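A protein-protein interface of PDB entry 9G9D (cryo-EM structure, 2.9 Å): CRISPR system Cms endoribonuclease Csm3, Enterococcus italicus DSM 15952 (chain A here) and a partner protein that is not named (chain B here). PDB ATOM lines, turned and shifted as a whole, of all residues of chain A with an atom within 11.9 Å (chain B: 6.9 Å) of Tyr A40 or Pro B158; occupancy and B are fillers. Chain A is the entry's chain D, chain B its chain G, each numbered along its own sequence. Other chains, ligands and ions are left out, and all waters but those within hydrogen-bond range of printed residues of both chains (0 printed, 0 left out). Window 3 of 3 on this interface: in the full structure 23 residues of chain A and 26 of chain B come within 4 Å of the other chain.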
ATOM      1  N   VAL A  35      16.394  30.689   5.971  1.00  0.00           N
ATOM      2  CA  VAL A  35      16.186  30.301   4.585  1.00  0.00           C
ATOM      3  C   VAL A  35      14.699  30.099   4.322  1.00  0.00           C
ATOM      4  O   VAL A  35      13.884  30.006   5.249  1.00  0.00           O
ATOM      5  CB  VAL A  35      16.982  29.030   4.240  1.00  0.00           C
ATOM      6  CG1 VAL A  35      18.427  29.375   3.991  1.00  0.00           C
ATOM      7  CG2 VAL A  35      16.866  28.013   5.359  1.00  0.00           C
ATOM      8  N   VAL A  36      14.340  30.045   3.039  1.00  0.00           N
ATOM      9  CA  VAL A  36      12.971  29.726   2.665  1.00  0.00           C
ATOM     10  C   VAL A  36      12.676  28.287   3.047  1.00  0.00           C
ATOM     11  O   VAL A  36      13.476  27.381   2.786  1.00  0.00           O
ATOM     12  CB  VAL A  36      12.760  29.965   1.164  1.00  0.00           C
ATOM     13  CG1 VAL A  36      11.316  29.709   0.781  1.00  0.00           C
ATOM     14  CG2 VAL A  36      13.149  31.375   0.808  1.00  0.00           C
ATOM     15  N   ARG A  37      11.521  28.068   3.671  1.00  0.00           N
ATOM     16  CA  ARG A  37      11.085  26.734   4.050  1.00  0.00           C
ATOM     17  C   ARG A  37       9.641  26.545   3.623  1.00  0.00           C
ATOM     18  O   ARG A  37       8.889  27.512   3.473  1.00  0.00           O
ATOM     19  CB  ARG A  37      11.203  26.494   5.559  1.00  0.00           C
ATOM     20  CG  ARG A  37      12.619  26.480   6.093  1.00  0.00           C
ATOM     21  CD  ARG A  37      12.636  26.025   7.537  1.00  0.00           C
ATOM     22  NE  ARG A  37      13.978  26.039   8.104  1.00  0.00           N
ATOM     23  CZ  ARG A  37      14.520  27.085   8.710  1.00  0.00           C
ATOM     24  NH1 ARG A  37      13.866  28.229   8.828  1.00  0.00           N
ATOM     25  NH2 ARG A  37      15.746  26.980   9.213  1.00  0.00           N
ATOM     26  N   ASP A  38       9.264  25.293   3.417  1.00  0.00           N
ATOM     27  CA  ASP A  38       7.867  24.977   3.177  1.00  0.00           C
ATOM     28  C   ASP A  38       7.058  25.327   4.422  1.00  0.00           C
ATOM     29  O   ASP A  38       7.450  24.948   5.533  1.00  0.00           O
ATOM     30  CB  ASP A  38       7.711  23.499   2.829  1.00  0.00           C
ATOM     31  CG  ASP A  38       6.298  23.139   2.440  1.00  0.00           C
ATOM     32  OD1 ASP A  38       5.774  23.735   1.476  1.00  0.00           O
ATOM     33  OD2 ASP A  38       5.713  22.250   3.091  1.00  0.00           O
ATOM     34  N   PRO A  39       5.952  26.064   4.291  1.00  0.00           N
ATOM     35  CA  PRO A  39       5.206  26.473   5.492  1.00  0.00           C
ATOM     36  C   PRO A  39       4.664  25.309   6.306  1.00  0.00           C
ATOM     37  O   PRO A  39       4.546  25.428   7.531  1.00  0.00           O
ATOM     38  CB  PRO A  39       4.076  27.341   4.921  1.00  0.00           C
ATOM     39  CG  PRO A  39       4.581  27.792   3.588  1.00  0.00           C
ATOM     40  CD  PRO A  39       5.379  26.639   3.066  1.00  0.00           C
ATOM     41  N   TYR A  40       4.331  24.187   5.668  1.00  0.00           N
ATOM     42  CA  TYR A  40       3.768  23.045   6.381  1.00  0.00           C
ATOM     43  C   TYR A  40       4.849  22.081   6.866  1.00  0.00           C
ATOM     44  O   TYR A  40       4.970  21.828   8.068  1.00  0.00           O
ATOM     45  CB  TYR A  40       2.764  22.307   5.491  1.00  0.00           C
ATOM     46  CG  TYR A  40       2.530  20.872   5.908  1.00  0.00           C
ATOM     47  CD1 TYR A  40       1.795  20.571   7.047  1.00  0.00           C
ATOM     48  CD2 TYR A  40       3.048  19.819   5.168  1.00  0.00           C
ATOM     49  CE1 TYR A  40       1.584  19.265   7.434  1.00  0.00           C
ATOM     50  CE2 TYR A  40       2.843  18.510   5.549  1.00  0.00           C
ATOM     51  CZ  TYR A  40       2.109  18.239   6.682  1.00  0.00           C
ATOM     52  OH  TYR A  40       1.898  16.937   7.067  1.00  0.00           O
ATOM     53  N   SER A  41       5.641  21.537   5.941  1.00  0.00           N
ATOM     54  CA  SER A  41       6.607  20.500   6.277  1.00  0.00           C
ATOM     55  C   SER A  41       7.899  21.050   6.861  1.00  0.00           C
ATOM     56  O   SER A  41       8.717  20.263   7.351  1.00  0.00           O
ATOM     57  CB  SER A  41       6.929  19.658   5.040  1.00  0.00           C
ATOM     58  OG  SER A  41       7.460  20.459   4.000  1.00  0.00           O
ATOM     59  N   ARG A  42       8.109  22.365   6.804  1.00  0.00           N
ATOM     60  CA  ARG A  42       9.297  23.029   7.340  1.00  0.00           C
ATOM     61  C   ARG A  42      10.585  22.562   6.673  1.00  0.00           C
ATOM     62  O   ARG A  42      11.681  22.859   7.157  1.00  0.00           O
ATOM     63  CB  ARG A  42       9.392  22.855   8.858  1.00  0.00           C
ATOM     64  CG  ARG A  42       8.176  23.368   9.599  1.00  0.00           C
ATOM     65  CD  ARG A  42       7.936  24.834   9.291  1.00  0.00           C
ATOM     66  NE  ARG A  42       8.968  25.686   9.870  1.00  0.00           N
ATOM     67  CZ  ARG A  42       9.036  26.999   9.701  1.00  0.00           C
ATOM     68  NH1 ARG A  42       8.159  27.645   8.950  1.00  0.00           N
ATOM     69  NH2 ARG A  42      10.009  27.681  10.299  1.00  0.00           N
ATOM     70  N   LEU A  43      10.482  21.837   5.570  1.00  0.00           N
ATOM     71  CA  LEU A  43      11.666  21.461   4.809  1.00  0.00           C
ATOM     72  C   LEU A  43      12.136  22.646   3.976  1.00  0.00           C
ATOM     73  O   LEU A  43      11.342  23.214   3.221  1.00  0.00           O
ATOM     74  CB  LEU A  43      11.374  20.276   3.897  1.00  0.00           C
ATOM     75  CG  LEU A  43      11.068  18.942   4.570  1.00  0.00           C
ATOM     76  CD1 LEU A  43      10.903  17.849   3.527  1.00  0.00           C
ATOM     77  CD2 LEU A  43      12.171  18.594   5.543  1.00  0.00           C
ATOM     78  N   PRO A  44      13.399  23.053   4.090  1.00  0.00           N
ATOM     79  CA  PRO A  44      13.887  24.167   3.271  1.00  0.00           C
ATOM     80  C   PRO A  44      13.751  23.854   1.789  1.00  0.00           C
ATOM     81  O   PRO A  44      13.933  22.715   1.357  1.00  0.00           O
ATOM     82  CB  PRO A  44      15.355  24.297   3.689  1.00  0.00           C
ATOM     83  CG  PRO A  44      15.704  22.960   4.242  1.00  0.00           C
ATOM     84  CD  PRO A  44      14.466  22.478   4.925  1.00  0.00           C
ATOM     85  N   ILE A  45      13.408  24.881   1.010  1.00  0.00           N
ATOM     86  CA  ILE A  45      13.175  24.722  -0.417  1.00  0.00           C
ATOM     87  C   ILE A  45      13.975  25.764  -1.183  1.00  0.00           C
ATOM     88  O   ILE A  45      14.474  26.743  -0.624  1.00  0.00           O
ATOM     89  CB  ILE A  45      11.680  24.835  -0.788  1.00  0.00           C
ATOM     90  CG1 ILE A  45      11.136  26.213  -0.406  1.00  0.00           C
ATOM     91  CG2 ILE A  45      10.877  23.728  -0.131  1.00  0.00           C
ATOM     92  CD1 ILE A  45       9.707  26.447  -0.833  1.00  0.00           C
ATOM     93  N   ASP A 100       9.234  25.285  -7.457  1.00  0.00           N
ATOM     94  CA  ASP A 100      10.207  25.455  -6.349  1.00  0.00           C
ATOM     95  C   ASP A 100      10.845  24.095  -6.071  1.00  0.00           C
ATOM     96  O   ASP A 100      10.114  23.090  -6.064  1.00  0.00           O
ATOM     97  CB  ASP A 100       9.537  25.974  -5.089  1.00  0.00           C
ATOM     98  CG  ASP A 100       8.874  27.339  -5.198  1.00  0.00           C
ATOM     99  OD1 ASP A 100       8.935  27.936  -6.292  1.00  0.00           O
ATOM    100  OD2 ASP A 100       8.307  27.797  -4.185  1.00  0.00           O
ATOM    101  N   PHE A 102      12.259  20.969  -4.039  1.00  0.00           N
ATOM    102  CA  PHE A 102      11.737  20.388  -2.772  1.00  0.00           C
ATOM    103  C   PHE A 102      12.819  19.512  -2.167  1.00  0.00           C
ATOM    104  O   PHE A 102      13.429  18.736  -2.926  1.00  0.00           O
ATOM    105  CB  PHE A 102      10.478  19.560  -3.038  1.00  0.00           C
ATOM    106  CG  PHE A 102       9.449  20.188  -3.970  1.00  0.00           C
ATOM    107  CD1 PHE A 102       8.521  21.105  -3.494  1.00  0.00           C
ATOM    108  CD2 PHE A 102       9.387  19.826  -5.311  1.00  0.00           C
ATOM    109  CE1 PHE A 102       7.576  21.664  -4.340  1.00  0.00           C
ATOM    110  CE2 PHE A 102       8.439  20.386  -6.153  1.00  0.00           C
ATOM    111  CZ  PHE A 102       7.535  21.301  -5.666  1.00  0.00           C
ATOM    112  N   PHE A 103      13.037  19.590  -0.851  1.00  0.00           N
ATOM    113  CA  PHE A 103      14.165  18.814  -0.272  1.00  0.00           C
ATOM    114  C   PHE A 103      13.858  17.368  -0.601  1.00  0.00           C
ATOM    115  O   PHE A 103      12.696  16.943  -0.432  1.00  0.00           O
ATOM    116  CB  PHE A 103      14.206  19.119   1.225  1.00  0.00           C
ATOM    117  CG  PHE A 103      15.435  18.661   1.995  1.00  0.00           C
ATOM    118  CD1 PHE A 103      15.507  17.382   2.535  1.00  0.00           C
ATOM    119  CD2 PHE A 103      16.500  19.527   2.214  1.00  0.00           C
ATOM    120  CE1 PHE A 103      16.623  16.977   3.248  1.00  0.00           C
ATOM    121  CE2 PHE A 103      17.612  19.116   2.930  1.00  0.00           C
ATOM    122  CZ  PHE A 103      17.672  17.842   3.444  1.00  0.00           C
ATOM    123  N   GLN A 108      16.522  13.416   2.825  1.00  0.00           N
ATOM    124  CA  GLN A 108      15.839  13.521   4.108  1.00  0.00           C
ATOM    125  C   GLN A 108      16.129  12.303   4.975  1.00  0.00           C
ATOM    126  O   GLN A 108      16.357  12.426   6.182  1.00  0.00           O
ATOM    127  CB  GLN A 108      14.337  13.693   3.887  1.00  0.00           C
ATOM    128  CG  GLN A 108      13.601  14.234   5.092  1.00  0.00           C
ATOM    129  CD  GLN A 108      12.193  14.674   4.763  1.00  0.00           C
ATOM    130  OE1 GLN A 108      11.740  14.546   3.626  1.00  0.00           O
ATOM    131  NE2 GLN A 108      11.491  15.200   5.758  1.00  0.00           N
ATOM    132  N   TYR A 118      18.692  19.569   8.963  1.00  0.00           N
ATOM    133  CA  TYR A 118      18.561  19.843   7.538  1.00  0.00           C
ATOM    134  C   TYR A 118      19.257  21.141   7.148  1.00  0.00           C
ATOM    135  O   TYR A 118      19.723  21.280   6.012  1.00  0.00           O
ATOM    136  CB  TYR A 118      17.088  19.894   7.147  1.00  0.00           C
ATOM    137  CG  TYR A 118      16.352  18.602   7.396  1.00  0.00           C
ATOM    138  CD1 TYR A 118      16.994  17.380   7.266  1.00  0.00           C
ATOM    139  CD2 TYR A 118      15.018  18.604   7.769  1.00  0.00           C
ATOM    140  CE1 TYR A 118      16.327  16.197   7.495  1.00  0.00           C
ATOM    141  CE2 TYR A 118      14.343  17.424   8.001  1.00  0.00           C
ATOM    142  CZ  TYR A 118      15.003  16.224   7.861  1.00  0.00           C
ATOM    143  OH  TYR A 118      14.338  15.044   8.091  1.00  0.00           O
ATOM    144  N   THR B  12      -4.573  17.940  -6.322  1.00  0.00           N
ATOM    145  CA  THR B  12      -3.598  17.901  -5.244  1.00  0.00           C
ATOM    146  C   THR B  12      -2.382  18.702  -5.681  1.00  0.00           C
ATOM    147  O   THR B  12      -1.766  18.391  -6.705  1.00  0.00           O
ATOM    148  CB  THR B  12      -3.195  16.463  -4.911  1.00  0.00           C
ATOM    149  OG1 THR B  12      -2.173  16.030  -5.815  1.00  0.00           O
ATOM    150  CG2 THR B  12      -4.392  15.532  -5.041  1.00  0.00           C
ATOM    151  N   TYR B  66     -11.159  20.064   0.290  1.00  0.00           N
ATOM    152  CA  TYR B  66     -11.466  18.723   0.758  1.00  0.00           C
ATOM    153  C   TYR B  66     -10.270  18.167   1.513  1.00  0.00           C
ATOM    154  O   TYR B  66      -9.120  18.506   1.227  1.00  0.00           O
ATOM    155  CB  TYR B  66     -11.857  17.777  -0.393  1.00  0.00           C
ATOM    156  CG  TYR B  66     -10.709  17.220  -1.210  1.00  0.00           C
ATOM    157  CD1 TYR B  66     -10.048  16.063  -0.821  1.00  0.00           C
ATOM    158  CD2 TYR B  66     -10.317  17.828  -2.390  1.00  0.00           C
ATOM    159  CE1 TYR B  66      -9.013  15.548  -1.567  1.00  0.00           C
ATOM    160  CE2 TYR B  66      -9.283  17.315  -3.145  1.00  0.00           C
ATOM    161  CZ  TYR B  66      -8.635  16.177  -2.729  1.00  0.00           C
ATOM    162  OH  TYR B  66      -7.604  15.662  -3.478  1.00  0.00           O
ATOM    163  N   ASN B 125      -8.960  21.631   7.514  1.00  0.00           N
ATOM    164  CA  ASN B 125      -7.507  21.534   7.486  1.00  0.00           C
ATOM    165  C   ASN B 125      -7.010  21.574   6.053  1.00  0.00           C
ATOM    166  O   ASN B 125      -6.233  20.720   5.616  1.00  0.00           O
ATOM    167  CB  ASN B 125      -7.021  20.277   8.202  1.00  0.00           C
ATOM    168  CG  ASN B 125      -6.670  20.537   9.653  1.00  0.00           C
ATOM    169  OD1 ASN B 125      -6.962  21.605  10.190  1.00  0.00           O
ATOM    170  ND2 ASN B 125      -6.037  19.563  10.294  1.00  0.00           N
ATOM    171  N   LEU B 126      -7.489  22.558   5.289  1.00  0.00           N
ATOM    172  CA  LEU B 126      -7.115  22.657   3.882  1.00  0.00           C
ATOM    173  C   LEU B 126      -5.619  22.895   3.715  1.00  0.00           C
ATOM    174  O   LEU B 126      -4.963  22.216   2.920  1.00  0.00           O
ATOM    175  CB  LEU B 126      -7.909  23.773   3.211  1.00  0.00           C
ATOM    176  CG  LEU B 126      -7.676  23.879   1.708  1.00  0.00           C
ATOM    177  CD1 LEU B 126      -8.032  22.567   1.036  1.00  0.00           C
ATOM    178  CD2 LEU B 126      -8.476  25.024   1.122  1.00  0.00           C
ATOM    179  N   GLY B 127      -5.063  23.848   4.452  1.00  0.00           N
ATOM    180  CA  GLY B 127      -3.657  24.157   4.313  1.00  0.00           C
ATOM    181  C   GLY B 127      -3.313  25.442   5.035  1.00  0.00           C
ATOM    182  O   GLY B 127      -4.094  25.953   5.840  1.00  0.00           O
ATOM    183  N   LYS B 128      -2.122  25.950   4.731  1.00  0.00           N
ATOM    184  CA  LYS B 128      -1.588  27.141   5.379  1.00  0.00           C
ATOM    185  C   LYS B 128      -1.250  28.196   4.337  1.00  0.00           C
ATOM    186  O   LYS B 128      -0.639  27.888   3.306  1.00  0.00           O
ATOM    187  CB  LYS B 128      -0.352  26.805   6.213  1.00  0.00           C
ATOM    188  CG  LYS B 128       0.125  27.948   7.086  1.00  0.00           C
ATOM    189  CD  LYS B 128       1.238  27.499   8.013  1.00  0.00           C
ATOM    190  CE  LYS B 128       1.604  28.596   8.998  1.00  0.00           C
ATOM    191  NZ  LYS B 128       0.437  29.018   9.818  1.00  0.00           N
ATOM    192  N   THR B 155      -0.192  26.608   0.724  1.00  0.00           N
ATOM    193  CA  THR B 155       0.309  25.245   0.617  1.00  0.00           C
ATOM    194  C   THR B 155      -0.676  24.306   1.296  1.00  0.00           C
ATOM    195  O   THR B 155      -1.009  24.489   2.473  1.00  0.00           O
ATOM    196  CB  THR B 155       1.705  25.118   1.228  1.00  0.00           C
ATOM    197  OG1 THR B 155       2.032  23.733   1.401  1.00  0.00           O
ATOM    198  CG2 THR B 155       1.780  25.835   2.564  1.00  0.00           C
ATOM    199  N   PHE B 156      -1.148  23.316   0.547  1.00  0.00           N
ATOM    200  CA  PHE B 156      -2.146  22.390   1.056  1.00  0.00           C
ATOM    201  C   PHE B 156      -1.493  21.285   1.872  1.00  0.00           C
ATOM    202  O   PHE B 156      -0.384  20.832   1.575  1.00  0.00           O
ATOM    203  CB  PHE B 156      -2.939  21.780  -0.097  1.00  0.00           C
ATOM    204  CG  PHE B 156      -3.693  22.786  -0.911  1.00  0.00           C
ATOM    205  CD1 PHE B 156      -3.067  23.492  -1.920  1.00  0.00           C
ATOM    206  CD2 PHE B 156      -5.031  23.018  -0.674  1.00  0.00           C
ATOM    207  CE1 PHE B 156      -3.763  24.418  -2.670  1.00  0.00           C
ATOM    208  CE2 PHE B 156      -5.727  23.936  -1.418  1.00  0.00           C
ATOM    209  CZ  PHE B 156      -5.094  24.637  -2.419  1.00  0.00           C
ATOM    210  N   TYR B 157      -2.198  20.848   2.910  1.00  0.00           N
ATOM    211  CA  TYR B 157      -1.740  19.710   3.683  1.00  0.00           C
ATOM    212  C   TYR B 157      -1.780  18.457   2.808  1.00  0.00           C
ATOM    213  O   TYR B 157      -2.555  18.390   1.851  1.00  0.00           O
ATOM    214  CB  TYR B 157      -2.604  19.537   4.927  1.00  0.00           C
ATOM    215  CG  TYR B 157      -2.441  20.660   5.924  1.00  0.00           C
ATOM    216  CD1 TYR B 157      -1.324  21.482   5.893  1.00  0.00           C
ATOM    217  CD2 TYR B 157      -3.400  20.897   6.897  1.00  0.00           C
ATOM    218  CE1 TYR B 157      -1.168  22.509   6.801  1.00  0.00           C
ATOM    219  CE2 TYR B 157      -3.252  21.923   7.810  1.00  0.00           C
ATOM    220  CZ  TYR B 157      -2.133  22.725   7.756  1.00  0.00           C
ATOM    221  OH  TYR B 157      -1.979  23.748   8.662  1.00  0.00           O
ATOM    222  N   PRO B 158      -0.938  17.460   3.100  1.00  0.00           N
ATOM    223  CA  PRO B 158      -0.762  16.356   2.137  1.00  0.00           C
ATOM    224  C   PRO B 158      -2.044  15.615   1.805  1.00  0.00           C
ATOM    225  O   PRO B 158      -2.226  15.188   0.659  1.00  0.00           O
ATOM    226  CB  PRO B 158       0.260  15.447   2.835  1.00  0.00           C
ATOM    227  CG  PRO B 158       0.165  15.797   4.276  1.00  0.00           C
ATOM    228  CD  PRO B 158      -0.137  17.256   4.318  1.00  0.00           C
ATOM    229  N   GLU B 159      -2.942  15.450   2.776  1.00  0.00           N
ATOM    230  CA  GLU B 159      -4.214  14.798   2.494  1.00  0.00           C
ATOM    231  C   GLU B 159      -5.176  15.743   1.785  1.00  0.00           C
ATOM    232  O   GLU B 159      -5.981  15.311   0.952  1.00  0.00           O
ATOM    233  CB  GLU B 159      -4.828  14.279   3.792  1.00  0.00           C
ATOM    234  CG  GLU B 159      -3.820  13.674   4.758  1.00  0.00           C
ATOM    235  CD  GLU B 159      -3.359  12.285   4.354  1.00  0.00           C
ATOM    236  OE1 GLU B 159      -3.818  11.772   3.311  1.00  0.00           O
ATOM    237  OE2 GLU B 159      -2.538  11.699   5.092  1.00  0.00           O
ATOM    238  N   SER B 160      -5.107  17.034   2.100  1.00  0.00           N
ATOM    239  CA  SER B 160      -6.086  17.988   1.598  1.00  0.00           C
ATOM    240  C   SER B 160      -5.831  18.342   0.139  1.00  0.00           C
ATOM    241  O   SER B 160      -4.758  18.079  -0.407  1.00  0.00           O
ATOM    242  CB  SER B 160      -6.065  19.258   2.449  1.00  0.00           C
ATOM    243  OG  SER B 160      -6.289  18.959   3.815  1.00  0.00           O
ATOM    244  N   GLY B 161      -6.832  18.955  -0.485  1.00  0.00           N
ATOM    245  CA  GLY B 161      -6.718  19.425  -1.853  1.00  0.00           C
ATOM    246  C   GLY B 161      -7.944  20.235  -2.213  1.00  0.00           C
ATOM    247  O   GLY B 161      -8.799  20.510  -1.366  1.00  0.00           O
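N of Lys B128 is in hydrogen-bond range of O of Thr B155 (2.9 Å). OD2 of Asp A38 sits at hydrogen-bond distance from OG of Ser A41 (2.7 Å). The backbone carbonyl oxygen of Leu B126 sits at hydrogen-bond distance from the backbone NH of Tyr B157 (3.1 Å). The backbone carbonyl oxygen of Leu A43 lies within hydrogen-bond range of the backbone NH of Asp A38, at 2.9 Å.
Among the printed residues, pairs that only touch across the chains: Asp A38 with Thr B155, Pro A39 with Lys B128, Pro A39 with Thr B155, Tyr A40 with Tyr B157 and Tyr A40 with Pro B158.
Of chain A, only Tyr A40 (3.4 Å) comes within 4 Å of Pro B158. Gly B127 touches none of the printed residues of chain A. Lys B128 touches just one residue of chain A: Pro A39. Thr B155 touches just these residues of chain A: Asp A38 and Pro A39. No residue of chain A comes within 4 Å of Glu B159. No residue of chain A comes within 4 Å of Ser B160. Of the printed residues of chain B, Asp A38 touches Thr B155. Of the printed residues of chain B, Pro A39 touches Lys B128 and Thr B155. Asn B125 touches none of the printed residues of chain A. Ile A45 touches none of the printed residues of chain B. The nearest residue of chain A that does not touch Pro B158 is Ser A41 (7.4 Å). The nearest printed residue of chain B that does not touch Asp A38 is Phe B156 (6.4 Å).
Of the 16 printed residues of chain A, 3 touch a printed residue of chain B. Among the printed residues, 5 pairs touch across the chains.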
